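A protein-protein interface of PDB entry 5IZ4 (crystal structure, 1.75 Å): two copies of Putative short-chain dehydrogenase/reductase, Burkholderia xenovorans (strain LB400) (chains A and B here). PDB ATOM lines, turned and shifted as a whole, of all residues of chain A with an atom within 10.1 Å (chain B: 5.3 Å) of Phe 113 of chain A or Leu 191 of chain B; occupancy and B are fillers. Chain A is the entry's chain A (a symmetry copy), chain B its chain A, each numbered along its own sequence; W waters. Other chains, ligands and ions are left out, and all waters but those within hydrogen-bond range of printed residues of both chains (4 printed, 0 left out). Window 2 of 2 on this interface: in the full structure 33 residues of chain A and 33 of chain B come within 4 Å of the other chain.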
ATOM      1  N   ILE A 108      -6.919 -18.674  30.079  1.00  0.00           N
ATOM      2  CA  ILE A 108      -7.093 -20.119  30.224  1.00  0.00           C
ATOM      3  C   ILE A 108      -6.296 -20.775  29.105  1.00  0.00           C
ATOM      4  O   ILE A 108      -6.576 -20.496  27.935  1.00  0.00           O
ATOM      5  CB  ILE A 108      -8.566 -20.540  30.118  1.00  0.00           C
ATOM      6  CG1 ILE A 108      -9.453 -19.731  31.067  1.00  0.00           C
ATOM      7  CG2 ILE A 108      -8.707 -22.030  30.386  1.00  0.00           C
ATOM      8  CD1 ILE A 108     -10.938 -19.914  30.780  1.00  0.00           C
ATOM      9  N   PRO A 109      -5.324 -21.640  29.396  1.00  0.00           N
ATOM     10  CA  PRO A 109      -4.552 -22.271  28.314  1.00  0.00           C
ATOM     11  C   PRO A 109      -5.460 -22.985  27.320  1.00  0.00           C
ATOM     12  O   PRO A 109      -6.422 -23.655  27.704  1.00  0.00           O
ATOM     13  CB  PRO A 109      -3.646 -23.256  29.056  1.00  0.00           C
ATOM     14  CG  PRO A 109      -3.498 -22.655  30.436  1.00  0.00           C
ATOM     15  CD  PRO A 109      -4.832 -22.024  30.730  1.00  0.00           C
ATOM     16  N   HIS A 110      -5.145 -22.826  26.027  1.00  0.00           N
ATOM     17  CA  HIS A 110      -5.996 -23.379  24.979  1.00  0.00           C
ATOM     18  C   HIS A 110      -6.014 -24.901  24.989  1.00  0.00           C
ATOM     19  O   HIS A 110      -6.947 -25.502  24.440  1.00  0.00           O
ATOM     20  CB  HIS A 110      -5.542 -22.896  23.592  1.00  0.00           C
ATOM     21  CG  HIS A 110      -5.823 -21.450  23.310  1.00  0.00           C
ATOM     22  ND1 HIS A 110      -6.436 -21.028  22.146  1.00  0.00           N
ATOM     23  CD2 HIS A 110      -5.532 -20.324  24.010  1.00  0.00           C
ATOM     24  CE1 HIS A 110      -6.530 -19.709  22.154  1.00  0.00           C
ATOM     25  NE2 HIS A 110      -5.996 -19.257  23.276  1.00  0.00           N
ATOM     26  N   ASN A 111      -5.003 -25.536  25.582  1.00  0.00           N
ATOM     27  CA  ASN A 111      -4.946 -26.988  25.678  1.00  0.00           C
ATOM     28  C   ASN A 111      -5.496 -27.517  26.995  1.00  0.00           C
ATOM     29  O   ASN A 111      -5.527 -28.734  27.193  1.00  0.00           O
ATOM     30  CB  ASN A 111      -3.505 -27.477  25.485  1.00  0.00           C
ATOM     31  CG  ASN A 111      -2.533 -26.840  26.463  1.00  0.00           C
ATOM     32  OD1 ASN A 111      -2.725 -25.702  26.895  1.00  0.00           O
ATOM     33  ND2 ASN A 111      -1.472 -27.568  26.805  1.00  0.00           N
ATOM     34  N   ALA A 112      -5.932 -26.642  27.899  1.00  0.00           N
ATOM     35  CA  ALA A 112      -6.587 -27.076  29.132  1.00  0.00           C
ATOM     36  C   ALA A 112      -8.094 -27.153  28.884  1.00  0.00           C
ATOM     37  O   ALA A 112      -8.878 -26.326  29.347  1.00  0.00           O
ATOM     38  CB  ALA A 112      -6.251 -26.129  30.275  1.00  0.00           C
ATOM     39  N   PHE A 113      -8.485 -28.168  28.098  1.00  0.00           N
ATOM     40  CA  PHE A 113      -9.881 -28.290  27.676  1.00  0.00           C
ATOM     41  C   PHE A 113     -10.832 -28.375  28.855  1.00  0.00           C
ATOM     42  O   PHE A 113     -11.973 -27.910  28.762  1.00  0.00           O
ATOM     43  CB  PHE A 113     -10.065 -29.520  26.787  1.00  0.00           C
ATOM     44  CG  PHE A 113      -9.355 -29.408  25.488  1.00  0.00           C
ATOM     45  CD1 PHE A 113      -9.968 -28.798  24.403  1.00  0.00           C
ATOM     46  CD2 PHE A 113      -8.060 -29.874  25.353  1.00  0.00           C
ATOM     47  CE1 PHE A 113      -9.302 -28.677  23.201  1.00  0.00           C
ATOM     48  CE2 PHE A 113      -7.389 -29.749  24.149  1.00  0.00           C
ATOM     49  CZ  PHE A 113      -8.014 -29.147  23.078  1.00  0.00           C
ATOM     50  N   ASP A 114     -10.385 -28.959  29.966  1.00  0.00           N
ATOM     51  CA  ASP A 114     -11.122 -29.208  31.192  1.00  0.00           C
ATOM     52  C   ASP A 114     -11.292 -27.969  32.058  1.00  0.00           C
ATOM     53  O   ASP A 114     -11.891 -28.066  33.132  1.00  0.00           O
ATOM     54  CB  ASP A 114     -10.393 -30.294  32.004  1.00  0.00           C
ATOM     55  CG  ASP A 114      -8.948 -29.898  32.390  1.00  0.00           C
ATOM     56  OD1 ASP A 114      -8.217 -29.273  31.580  1.00  0.00           O
ATOM     57  OD2 ASP A 114      -8.530 -30.231  33.518  1.00  0.00           O
ATOM     58  N   GLN A 115     -10.714 -26.835  31.669  1.00  0.00           N
ATOM     59  CA  GLN A 115     -10.712 -25.637  32.501  1.00  0.00           C
ATOM     60  C   GLN A 115     -11.443 -24.469  31.854  1.00  0.00           C
ATOM     61  O   GLN A 115     -11.321 -23.334  32.323  1.00  0.00           O
ATOM     62  CB  GLN A 115      -9.274 -25.257  32.856  1.00  0.00           C
ATOM     63  CG  GLN A 115      -8.563 -26.405  33.563  1.00  0.00           C
ATOM     64  CD  GLN A 115      -7.271 -25.996  34.241  1.00  0.00           C
ATOM     65  OE1 GLN A 115      -6.582 -25.082  33.796  1.00  0.00           O
ATOM     66  NE2 GLN A 115      -6.938 -26.680  35.332  1.00  0.00           N
ATOM     67  N   ILE A 116     -12.211 -24.717  30.803  1.00  0.00           N
ATOM     68  CA  ILE A 116     -13.098 -23.717  30.231  1.00  0.00           C
ATOM     69  C   ILE A 116     -14.469 -24.366  30.079  1.00  0.00           C
ATOM     70  O   ILE A 116     -14.581 -25.595  30.007  1.00  0.00           O
ATOM     71  CB  ILE A 116     -12.543 -23.180  28.889  1.00  0.00           C
ATOM     72  CG1 ILE A 116     -13.230 -21.866  28.500  1.00  0.00           C
ATOM     73  CG2 ILE A 116     -12.676 -24.227  27.785  1.00  0.00           C
ATOM     74  CD1 ILE A 116     -12.515 -21.105  27.383  1.00  0.00           C
ATOM     75  N   ASP A 117     -15.525 -23.549  30.089  1.00  0.00           N
ATOM     76  CA  ASP A 117     -16.877 -24.096  29.951  1.00  0.00           C
ATOM     77  C   ASP A 117     -17.748 -23.153  29.136  1.00  0.00           C
ATOM     78  O   ASP A 117     -17.339 -22.044  28.778  1.00  0.00           O
ATOM     79  CB  ASP A 117     -17.529 -24.378  31.313  1.00  0.00           C
ATOM     80  CG  ASP A 117     -17.550 -23.167  32.218  1.00  0.00           C
ATOM     81  OD1 ASP A 117     -17.178 -22.059  31.776  1.00  0.00           O
ATOM     82  OD2 ASP A 117     -17.950 -23.326  33.383  1.00  0.00           O
ATOM     83  N   ASP A 118     -18.977 -23.606  28.861  1.00  0.00           N
ATOM     84  CA  ASP A 118     -19.901 -22.793  28.078  1.00  0.00           C
ATOM     85  C   ASP A 118     -20.161 -21.446  28.744  1.00  0.00           C
ATOM     86  O   ASP A 118     -20.287 -20.425  28.055  1.00  0.00           O
ATOM     87  CB  ASP A 118     -21.214 -23.550  27.821  1.00  0.00           C
ATOM     88  CG  ASP A 118     -21.901 -24.075  29.093  1.00  0.00           C
ATOM     89  OD1 ASP A 118     -21.300 -24.119  30.189  1.00  0.00           O
ATOM     90  OD2 ASP A 118     -23.081 -24.484  28.974  1.00  0.00           O
ATOM     91  N   GLU A 120     -18.113 -19.505  30.231  1.00  0.00           N
ATOM     92  CA  GLU A 120     -17.065 -18.557  29.880  1.00  0.00           C
ATOM     93  C   GLU A 120     -17.138 -18.168  28.409  1.00  0.00           C
ATOM     94  O   GLU A 120     -16.931 -16.997  28.069  1.00  0.00           O
ATOM     95  CB  GLU A 120     -15.696 -19.139  30.236  1.00  0.00           C
ATOM     96  CG  GLU A 120     -14.517 -18.251  29.863  1.00  0.00           C
ATOM     97  CD  GLU A 120     -14.447 -16.961  30.667  1.00  0.00           C
ATOM     98  OE1 GLU A 120     -15.198 -16.805  31.677  1.00  0.00           O
ATOM     99  OE2 GLU A 120     -13.632 -16.093  30.276  1.00  0.00           O
ATOM    100  N   PHE A 121     -17.476 -19.116  27.529  1.00  0.00           N
ATOM    101  CA  PHE A 121     -17.675 -18.759  26.127  1.00  0.00           C
ATOM    102  C   PHE A 121     -18.747 -17.685  26.011  1.00  0.00           C
ATOM    103  O   PHE A 121     -18.569 -16.687  25.301  1.00  0.00           O
ATOM    104  CB  PHE A 121     -18.073 -19.984  25.291  1.00  0.00           C
ATOM    105  CG  PHE A 121     -16.917 -20.843  24.824  1.00  0.00           C
ATOM    106  CD1 PHE A 121     -16.512 -21.948  25.563  1.00  0.00           C
ATOM    107  CD2 PHE A 121     -16.264 -20.569  23.630  1.00  0.00           C
ATOM    108  CE1 PHE A 121     -15.477 -22.758  25.134  1.00  0.00           C
ATOM    109  CE2 PHE A 121     -15.215 -21.380  23.189  1.00  0.00           C
ATOM    110  CZ  PHE A 121     -14.820 -22.472  23.943  1.00  0.00           C
ATOM    111  N   GLY A 166      -6.157 -17.549  16.141  1.00  0.00           N
ATOM    112  CA  GLY A 166      -6.590 -18.505  17.154  1.00  0.00           C
ATOM    113  C   GLY A 166      -5.687 -18.630  18.365  1.00  0.00           C
ATOM    114  O   GLY A 166      -5.717 -19.657  19.056  1.00  0.00           O
ATOM    115  N   ILE A 171      -9.313 -19.693  24.303  1.00  0.00           N
ATOM    116  CA  ILE A 171      -9.985 -20.061  23.063  1.00  0.00           C
ATOM    117  C   ILE A 171     -11.351 -19.382  22.969  1.00  0.00           C
ATOM    118  O   ILE A 171     -11.828 -19.088  21.863  1.00  0.00           O
ATOM    119  CB  ILE A 171     -10.079 -21.597  22.949  1.00  0.00           C
ATOM    120  CG1 ILE A 171     -10.417 -22.007  21.509  1.00  0.00           C
ATOM    121  CG2 ILE A 171     -11.089 -22.178  23.949  1.00  0.00           C
ATOM    122  CD1 ILE A 171     -10.542 -23.512  21.314  1.00  0.00           C
ATOM    123  N   ALA A 172     -12.002 -19.111  24.112  1.00  0.00           N
ATOM    124  CA  ALA A 172     -13.260 -18.365  24.078  1.00  0.00           C
ATOM    125  C   ALA A 172     -13.031 -16.927  23.634  1.00  0.00           C
ATOM    126  O   ALA A 172     -13.850 -16.350  22.906  1.00  0.00           O
ATOM    127  CB  ALA A 172     -13.941 -18.402  25.454  1.00  0.00           C
ATOM    128  N   TYR B 133     -17.541 -26.934  19.899  1.00  0.00           N
ATOM    129  CA  TYR B 133     -16.414 -27.115  20.809  1.00  0.00           C
ATOM    130  C   TYR B 133     -16.668 -28.249  21.803  1.00  0.00           C
ATOM    131  O   TYR B 133     -15.778 -29.071  22.068  1.00  0.00           O
ATOM    132  CB  TYR B 133     -16.131 -25.817  21.560  1.00  0.00           C
ATOM    133  CG  TYR B 133     -15.062 -25.988  22.610  1.00  0.00           C
ATOM    134  CD1 TYR B 133     -15.395 -26.239  23.939  1.00  0.00           C
ATOM    135  CD2 TYR B 133     -13.713 -25.925  22.268  1.00  0.00           C
ATOM    136  CE1 TYR B 133     -14.419 -26.414  24.906  1.00  0.00           C
ATOM    137  CE2 TYR B 133     -12.724 -26.094  23.220  1.00  0.00           C
ATOM    138  CZ  TYR B 133     -13.086 -26.344  24.543  1.00  0.00           C
ATOM    139  OH  TYR B 133     -12.107 -26.518  25.486  1.00  0.00           O
ATOM    140  N   THR B 136     -16.333 -31.652  20.154  1.00  0.00           N
ATOM    141  CA  THR B 136     -14.934 -31.926  19.853  1.00  0.00           C
ATOM    142  C   THR B 136     -14.169 -32.284  21.120  1.00  0.00           C
ATOM    143  O   THR B 136     -13.457 -33.294  21.160  1.00  0.00           O
ATOM    144  CB  THR B 136     -14.300 -30.718  19.169  1.00  0.00           C
ATOM    145  OG1 THR B 136     -15.015 -30.403  17.963  1.00  0.00           O
ATOM    146  CG2 THR B 136     -12.863 -31.032  18.811  1.00  0.00           C
ATOM    147  N   ARG B 137     -14.326 -31.472  22.173  1.00  0.00           N
ATOM    148  CA  ARG B 137     -13.667 -31.749  23.448  1.00  0.00           C
ATOM    149  C   ARG B 137     -14.029 -33.129  23.978  1.00  0.00           C
ATOM    150  O   ARG B 137     -13.160 -33.851  24.487  1.00  0.00           O
ATOM    151  CB  ARG B 137     -14.033 -30.684  24.486  1.00  0.00           C
ATOM    152  CG  ARG B 137     -13.508 -31.010  25.892  1.00  0.00           C
ATOM    153  CD  ARG B 137     -13.771 -29.885  26.917  1.00  0.00           C
ATOM    154  NE  ARG B 137     -15.200 -29.641  27.140  1.00  0.00           N
ATOM    155  CZ  ARG B 137     -15.686 -28.600  27.804  1.00  0.00           C
ATOM    156  NH1 ARG B 137     -14.861 -27.701  28.334  1.00  0.00           N
ATOM    157  NH2 ARG B 137     -17.004 -28.461  27.951  1.00  0.00           N
ATOM    158  N   VAL B 140     -12.067 -35.781  22.052  1.00  0.00           N
ATOM    159  CA  VAL B 140     -10.604 -35.672  21.946  1.00  0.00           C
ATOM    160  C   VAL B 140      -9.878 -36.862  22.563  1.00  0.00           C
ATOM    161  O   VAL B 140      -8.939 -37.380  21.925  1.00  0.00           O
ATOM    162  CB  VAL B 140     -10.138 -34.324  22.533  1.00  0.00           C
ATOM    163  CG1 VAL B 140      -8.703 -34.417  23.031  1.00  0.00           C
ATOM    164  CG2 VAL B 140     -10.283 -33.207  21.503  1.00  0.00           C
ATOM    165  N   ARG B 144      -7.458 -38.952  20.082  1.00  0.00           N
ATOM    166  CA  ARG B 144      -6.012 -39.029  20.256  1.00  0.00           C
ATOM    167  C   ARG B 144      -5.556 -40.475  20.405  1.00  0.00           C
ATOM    168  O   ARG B 144      -4.523 -40.871  19.852  1.00  0.00           O
ATOM    169  CB  ARG B 144      -5.595 -38.192  21.465  1.00  0.00           C
ATOM    170  CG  ARG B 144      -4.102 -38.081  21.626  1.00  0.00           C
ATOM    171  CD  ARG B 144      -3.725 -37.253  22.835  1.00  0.00           C
ATOM    172  NE  ARG B 144      -4.039 -35.835  22.681  1.00  0.00           N
ATOM    173  CZ  ARG B 144      -4.909 -35.180  23.440  1.00  0.00           C
ATOM    174  NH1 ARG B 144      -5.557 -35.816  24.406  1.00  0.00           N
ATOM    175  NH2 ARG B 144      -5.118 -33.888  23.248  1.00  0.00           N
ATOM    176  N   SER B 186      -7.312 -22.654  16.642  1.00  0.00           N
ATOM    177  CA  SER B 186      -6.814 -23.001  17.966  1.00  0.00           C
ATOM    178  C   SER B 186      -6.783 -24.511  18.151  1.00  0.00           C
ATOM    179  O   SER B 186      -5.797 -25.073  18.647  1.00  0.00           O
ATOM    180  CB  SER B 186      -7.683 -22.349  19.045  1.00  0.00           C
ATOM    181  OG  SER B 186      -7.255 -22.795  20.324  1.00  0.00           O
ATOM    182  N   LEU B 187      -7.873 -25.184  17.771  1.00  0.00           N
ATOM    183  CA  LEU B 187      -7.951 -26.630  17.943  1.00  0.00           C
ATOM    184  C   LEU B 187      -6.868 -27.330  17.134  1.00  0.00           C
ATOM    185  O   LEU B 187      -6.207 -28.250  17.630  1.00  0.00           O
ATOM    186  CB  LEU B 187      -9.334 -27.131  17.539  1.00  0.00           C
ATOM    187  CG  LEU B 187     -10.517 -26.749  18.452  1.00  0.00           C
ATOM    188  CD1 LEU B 187     -11.819 -27.192  17.797  1.00  0.00           C
ATOM    189  CD2 LEU B 187     -10.367 -27.355  19.843  1.00  0.00           C
ATOM    190  N   ALA B 188      -6.664 -26.900  15.886  1.00  0.00           N
ATOM    191  CA  ALA B 188      -5.611 -27.492  15.071  1.00  0.00           C
ATOM    192  C   ALA B 188      -4.248 -27.323  15.731  1.00  0.00           C
ATOM    193  O   ALA B 188      -3.450 -28.265  15.787  1.00  0.00           O
ATOM    194  CB  ALA B 188      -5.605 -26.868  13.673  1.00  0.00           C
ATOM    195  N   ARG B 189      -3.958 -26.115  16.223  1.00  0.00           N
ATOM    196  CA  ARG B 189      -2.653 -25.869  16.824  1.00  0.00           C
ATOM    197  C   ARG B 189      -2.455 -26.721  18.069  1.00  0.00           C
ATOM    198  O   ARG B 189      -1.365 -27.264  18.301  1.00  0.00           O
ATOM    199  CB  ARG B 189      -2.499 -24.385  17.160  1.00  0.00           C
ATOM    200  CG  ARG B 189      -1.140 -24.017  17.725  1.00  0.00           C
ATOM    201  CD  ARG B 189      -1.023 -22.528  18.032  1.00  0.00           C
ATOM    202  NE  ARG B 189      -1.024 -21.712  16.820  1.00  0.00           N
ATOM    203  CZ  ARG B 189      -2.057 -20.990  16.407  1.00  0.00           C
ATOM    204  NH1 ARG B 189      -3.188 -20.968  17.111  1.00  0.00           N
ATOM    205  NH2 ARG B 189      -1.960 -20.277  15.285  1.00  0.00           N
ATOM    206  N   ASN B 190      -3.492 -26.848  18.888  1.00  0.00           N
ATOM    207  CA  ASN B 190      -3.312 -27.480  20.183  1.00  0.00           C
ATOM    208  C   ASN B 190      -3.543 -28.988  20.181  1.00  0.00           C
ATOM    209  O   ASN B 190      -3.152 -29.655  21.147  1.00  0.00           O
ATOM    210  CB  ASN B 190      -4.229 -26.806  21.203  1.00  0.00           C
ATOM    211  CG  ASN B 190      -3.742 -25.428  21.562  1.00  0.00           C
ATOM    212  OD1 ASN B 190      -2.887 -25.276  22.438  1.00  0.00           O
ATOM    213  ND2 ASN B 190      -4.236 -24.418  20.857  1.00  0.00           N
ATOM    214  N   LEU B 191      -4.154 -29.545  19.141  1.00  0.00           N
ATOM    215  CA  LEU B 191      -4.329 -30.987  19.065  1.00  0.00           C
ATOM    216  C   LEU B 191      -3.324 -31.652  18.137  1.00  0.00           C
ATOM    217  O   LEU B 191      -3.259 -32.889  18.094  1.00  0.00           O
ATOM    218  CB  LEU B 191      -5.762 -31.326  18.631  1.00  0.00           C
ATOM    219  CG  LEU B 191      -6.849 -30.881  19.636  1.00  0.00           C
ATOM    220  CD1 LEU B 191      -8.242 -31.104  19.058  1.00  0.00           C
ATOM    221  CD2 LEU B 191      -6.709 -31.620  20.964  1.00  0.00           C
ATOM    222  N   ALA B 192      -2.540 -30.869  17.397  1.00  0.00           N
ATOM    223  CA  ALA B 192      -1.419 -31.438  16.671  1.00  0.00           C
ATOM    224  C   ALA B 192      -0.488 -32.139  17.657  1.00  0.00           C
ATOM    225  O   ALA B 192      -0.321 -31.682  18.789  1.00  0.00           O
ATOM    226  CB  ALA B 192      -0.650 -30.351  15.925  1.00  0.00           C
ATOM    227  N   PRO B 193       0.172 -33.230  17.247  1.00  0.00           N
ATOM    228  CA  PRO B 193       0.185 -33.801  15.896  1.00  0.00           C
ATOM    229  C   PRO B 193      -0.797 -34.945  15.686  1.00  0.00           C
ATOM    230  O   PRO B 193      -0.905 -35.423  14.554  1.00  0.00           O
ATOM    231  CB  PRO B 193       1.619 -34.315  15.771  1.00  0.00           C
ATOM    232  CG  PRO B 193       1.940 -34.769  17.148  1.00  0.00           C
ATOM    233  CD  PRO B 193       1.255 -33.790  18.079  1.00  0.00           C
ATOM    234  N   HIS B 194      -1.497 -35.358  16.750  1.00  0.00           N
ATOM    235  CA  HIS B 194      -2.296 -36.581  16.702  1.00  0.00           C
ATOM    236  C   HIS B 194      -3.639 -36.386  16.021  1.00  0.00           C
ATOM    237  O   HIS B 194      -4.187 -37.345  15.473  1.00  0.00           O
ATOM    238  CB  HIS B 194      -2.508 -37.123  18.111  1.00  0.00           C
ATOM    239  CG  HIS B 194      -1.235 -37.293  18.873  1.00  0.00           C
ATOM    240  ND1 HIS B 194      -0.829 -36.412  19.852  1.00  0.00           N
ATOM    241  CD2 HIS B 194      -0.258 -38.223  18.773  1.00  0.00           C
ATOM    242  CE1 HIS B 194       0.333 -36.806  20.341  1.00  0.00           C
ATOM    243  NE2 HIS B 194       0.701 -37.903  19.702  1.00  0.00           N
ATOM    244  N   ILE B 195      -4.182 -35.173  16.044  1.00  0.00           N
ATOM    245  CA  ILE B 195      -5.498 -34.883  15.479  1.00  0.00           C
ATOM    246  C   ILE B 195      -5.368 -33.674  14.566  1.00  0.00           C
ATOM    247  O   ILE B 195      -4.785 -32.659  14.960  1.00  0.00           O
ATOM    248  CB  ILE B 195      -6.548 -34.603  16.574  1.00  0.00           C
ATOM    249  CG1 ILE B 195      -6.595 -35.739  17.596  1.00  0.00           C
ATOM    250  CG2 ILE B 195      -7.921 -34.384  15.935  1.00  0.00           C
ATOM    251  CD1 ILE B 195      -7.340 -35.362  18.910  1.00  0.00           C
ATOM    252  N   VAL B 197      -7.483 -30.732  12.438  1.00  0.00           N
ATOM    253  CA  VAL B 197      -8.759 -30.033  12.571  1.00  0.00           C
ATOM    254  C   VAL B 197      -8.885 -29.060  11.411  1.00  0.00           C
ATOM    255  O   VAL B 197      -8.018 -28.193  11.226  1.00  0.00           O
ATOM    256  CB  VAL B 197      -8.886 -29.286  13.910  1.00  0.00           C
ATOM    257  CG1 VAL B 197     -10.331 -28.751  14.092  1.00  0.00           C
ATOM    258  CG2 VAL B 197      -8.503 -30.190  15.090  1.00  0.00           C
HETATM  259  O   HOH W   1      -3.813 -21.545  19.984  1.00  0.00           O
HETATM  260  O   HOH W   2     -19.064 -26.508  28.991  1.00  0.00           O
HETATM  261  O   HOH W   3      -7.453 -25.669  21.389  1.00  0.00           O
HETATM  262  O   HOH W   4      -9.735 -25.487  25.040  1.00  0.00           O
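O of Ser 186 of chain B sits at hydrogen-bond distance from ND2 of Asn 190 of chain B, 2.8 Å away. O of Gly 166 of chain A sits close to ND1 of His 110 of chain A (3.5 Å).
Pro 109 of chain A touches none of the printed residues of chain B. Of the printed residues of chain B, Asn 111 of chain A touches Asn 190 (3.8 Å). Of the printed residues of chain B, Phe 113 of chain A touches Tyr 133, Arg 137, Leu 187 and Leu 191. Printed residues of chain A within 4 Å of Tyr 133 of chain B: Phe 113 (3.3 Å), Ile 116 (3.3 Å), Phe 121 (3.7 Å) and Ile 171 (3.9 Å). Of chain A, only Phe 113 (3.8 Å) comes within 4 Å of Leu 187 of chain B. Of chain A, only His 110 and Asn 111 come within 4 Å of Asn 190 of chain B. Leu 191 of chain B touches just one residue of chain A: Phe 113. No residue of chain A comes within 4 Å of Ala 192 of chain B. No residue of chain A comes within 4 Å of Pro 193 of chain B. Ile 195 of chain B touches none of the printed residues of chain A. The nearest printed residue of chain B that does not touch Phe 113 of chain A is Arg 144 of chain B (4.8 Å).
Hydrophobic or aromatic side chains of chain B that line the printed part of chain A: Tyr 133, Leu 187 and Leu 191. Of the 16 printed residues of chain A, 7 touch a printed residue of chain B.
Water W4 lies within hydrogen-bond range of the side-chain hydroxyl (OH) of Tyr 133 of chain B (2.6 Å) and the backbone carbonyl oxygen (O) of His 110 of chain A (2.9 Å). Water W1 lies within hydrogen-bond range of O of Gly 166 of chain A (2.8 Å), NH1 of Arg 189 of chain B (3.0 Å), ND2 of Asn 190 of chain B (3.0 Å) and ND1 of His 110 of chain A (3.4 Å). Water W2 lies within hydrogen-bond range of the backbone NH (N) of Asp 118 of chain A (2.9 Å) and the guanidinium group (NH2) of Arg 137 of chain B (3.0 Å). Water W3 lies within hydrogen-bond range of the side-chain hydroxyl (OG) of Ser 186 of chain B (3.1 Å), the backbone carbonyl oxygen (O) of His 110 of chain A (3.1 Å) and the side-chain amide nitrogen (ND2) of Asn 190 of chain B (3.5 Å).
Among the printed residues, merely in contact across the chains: His 110 of chain A with Asn 190 of chain B, Asn 111 of chain A with Asn 190 of chain B, Phe 113 of chain A with Tyr 133 of chain B, Phe 113 of chain A with Leu 187 of chain B, Phe 113 of chain A with Leu 191 of chain B, Ile 116 of chain A with Tyr 133 of chain B, Phe 121 of chain A with Tyr 133 of chain B, Gly 166 of chain A with Ser 186 of chain B, Ile 171 of chain A with Tyr 133 of chain B and Ile 171 of chain A with Ser 186 of chain B.
NH1 of Arg 189 of chain B is in hydrogen-bond range of O of Gly 166 of chain A. The guanidinium group (NH1) of Arg 137 of chain B lies within hydrogen-bond range of the backbone carbonyl oxygen (O) of Ile 116 of chain A (2.7 Å). NH1 of Arg 137 of chain B lies within hydrogen-bond range of O of Phe 113 of chain A (2.9 Å). A ring nitrogen (ND1) of His 110 of chain A sits at hydrogen-bond distance from the side-chain hydroxyl (OG) of Ser 186 of chain B.
No position is printed for both chains. Of the 14 pairs that touch across the chains among the printed residues, none has its exchanged pair printed and touching as well.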
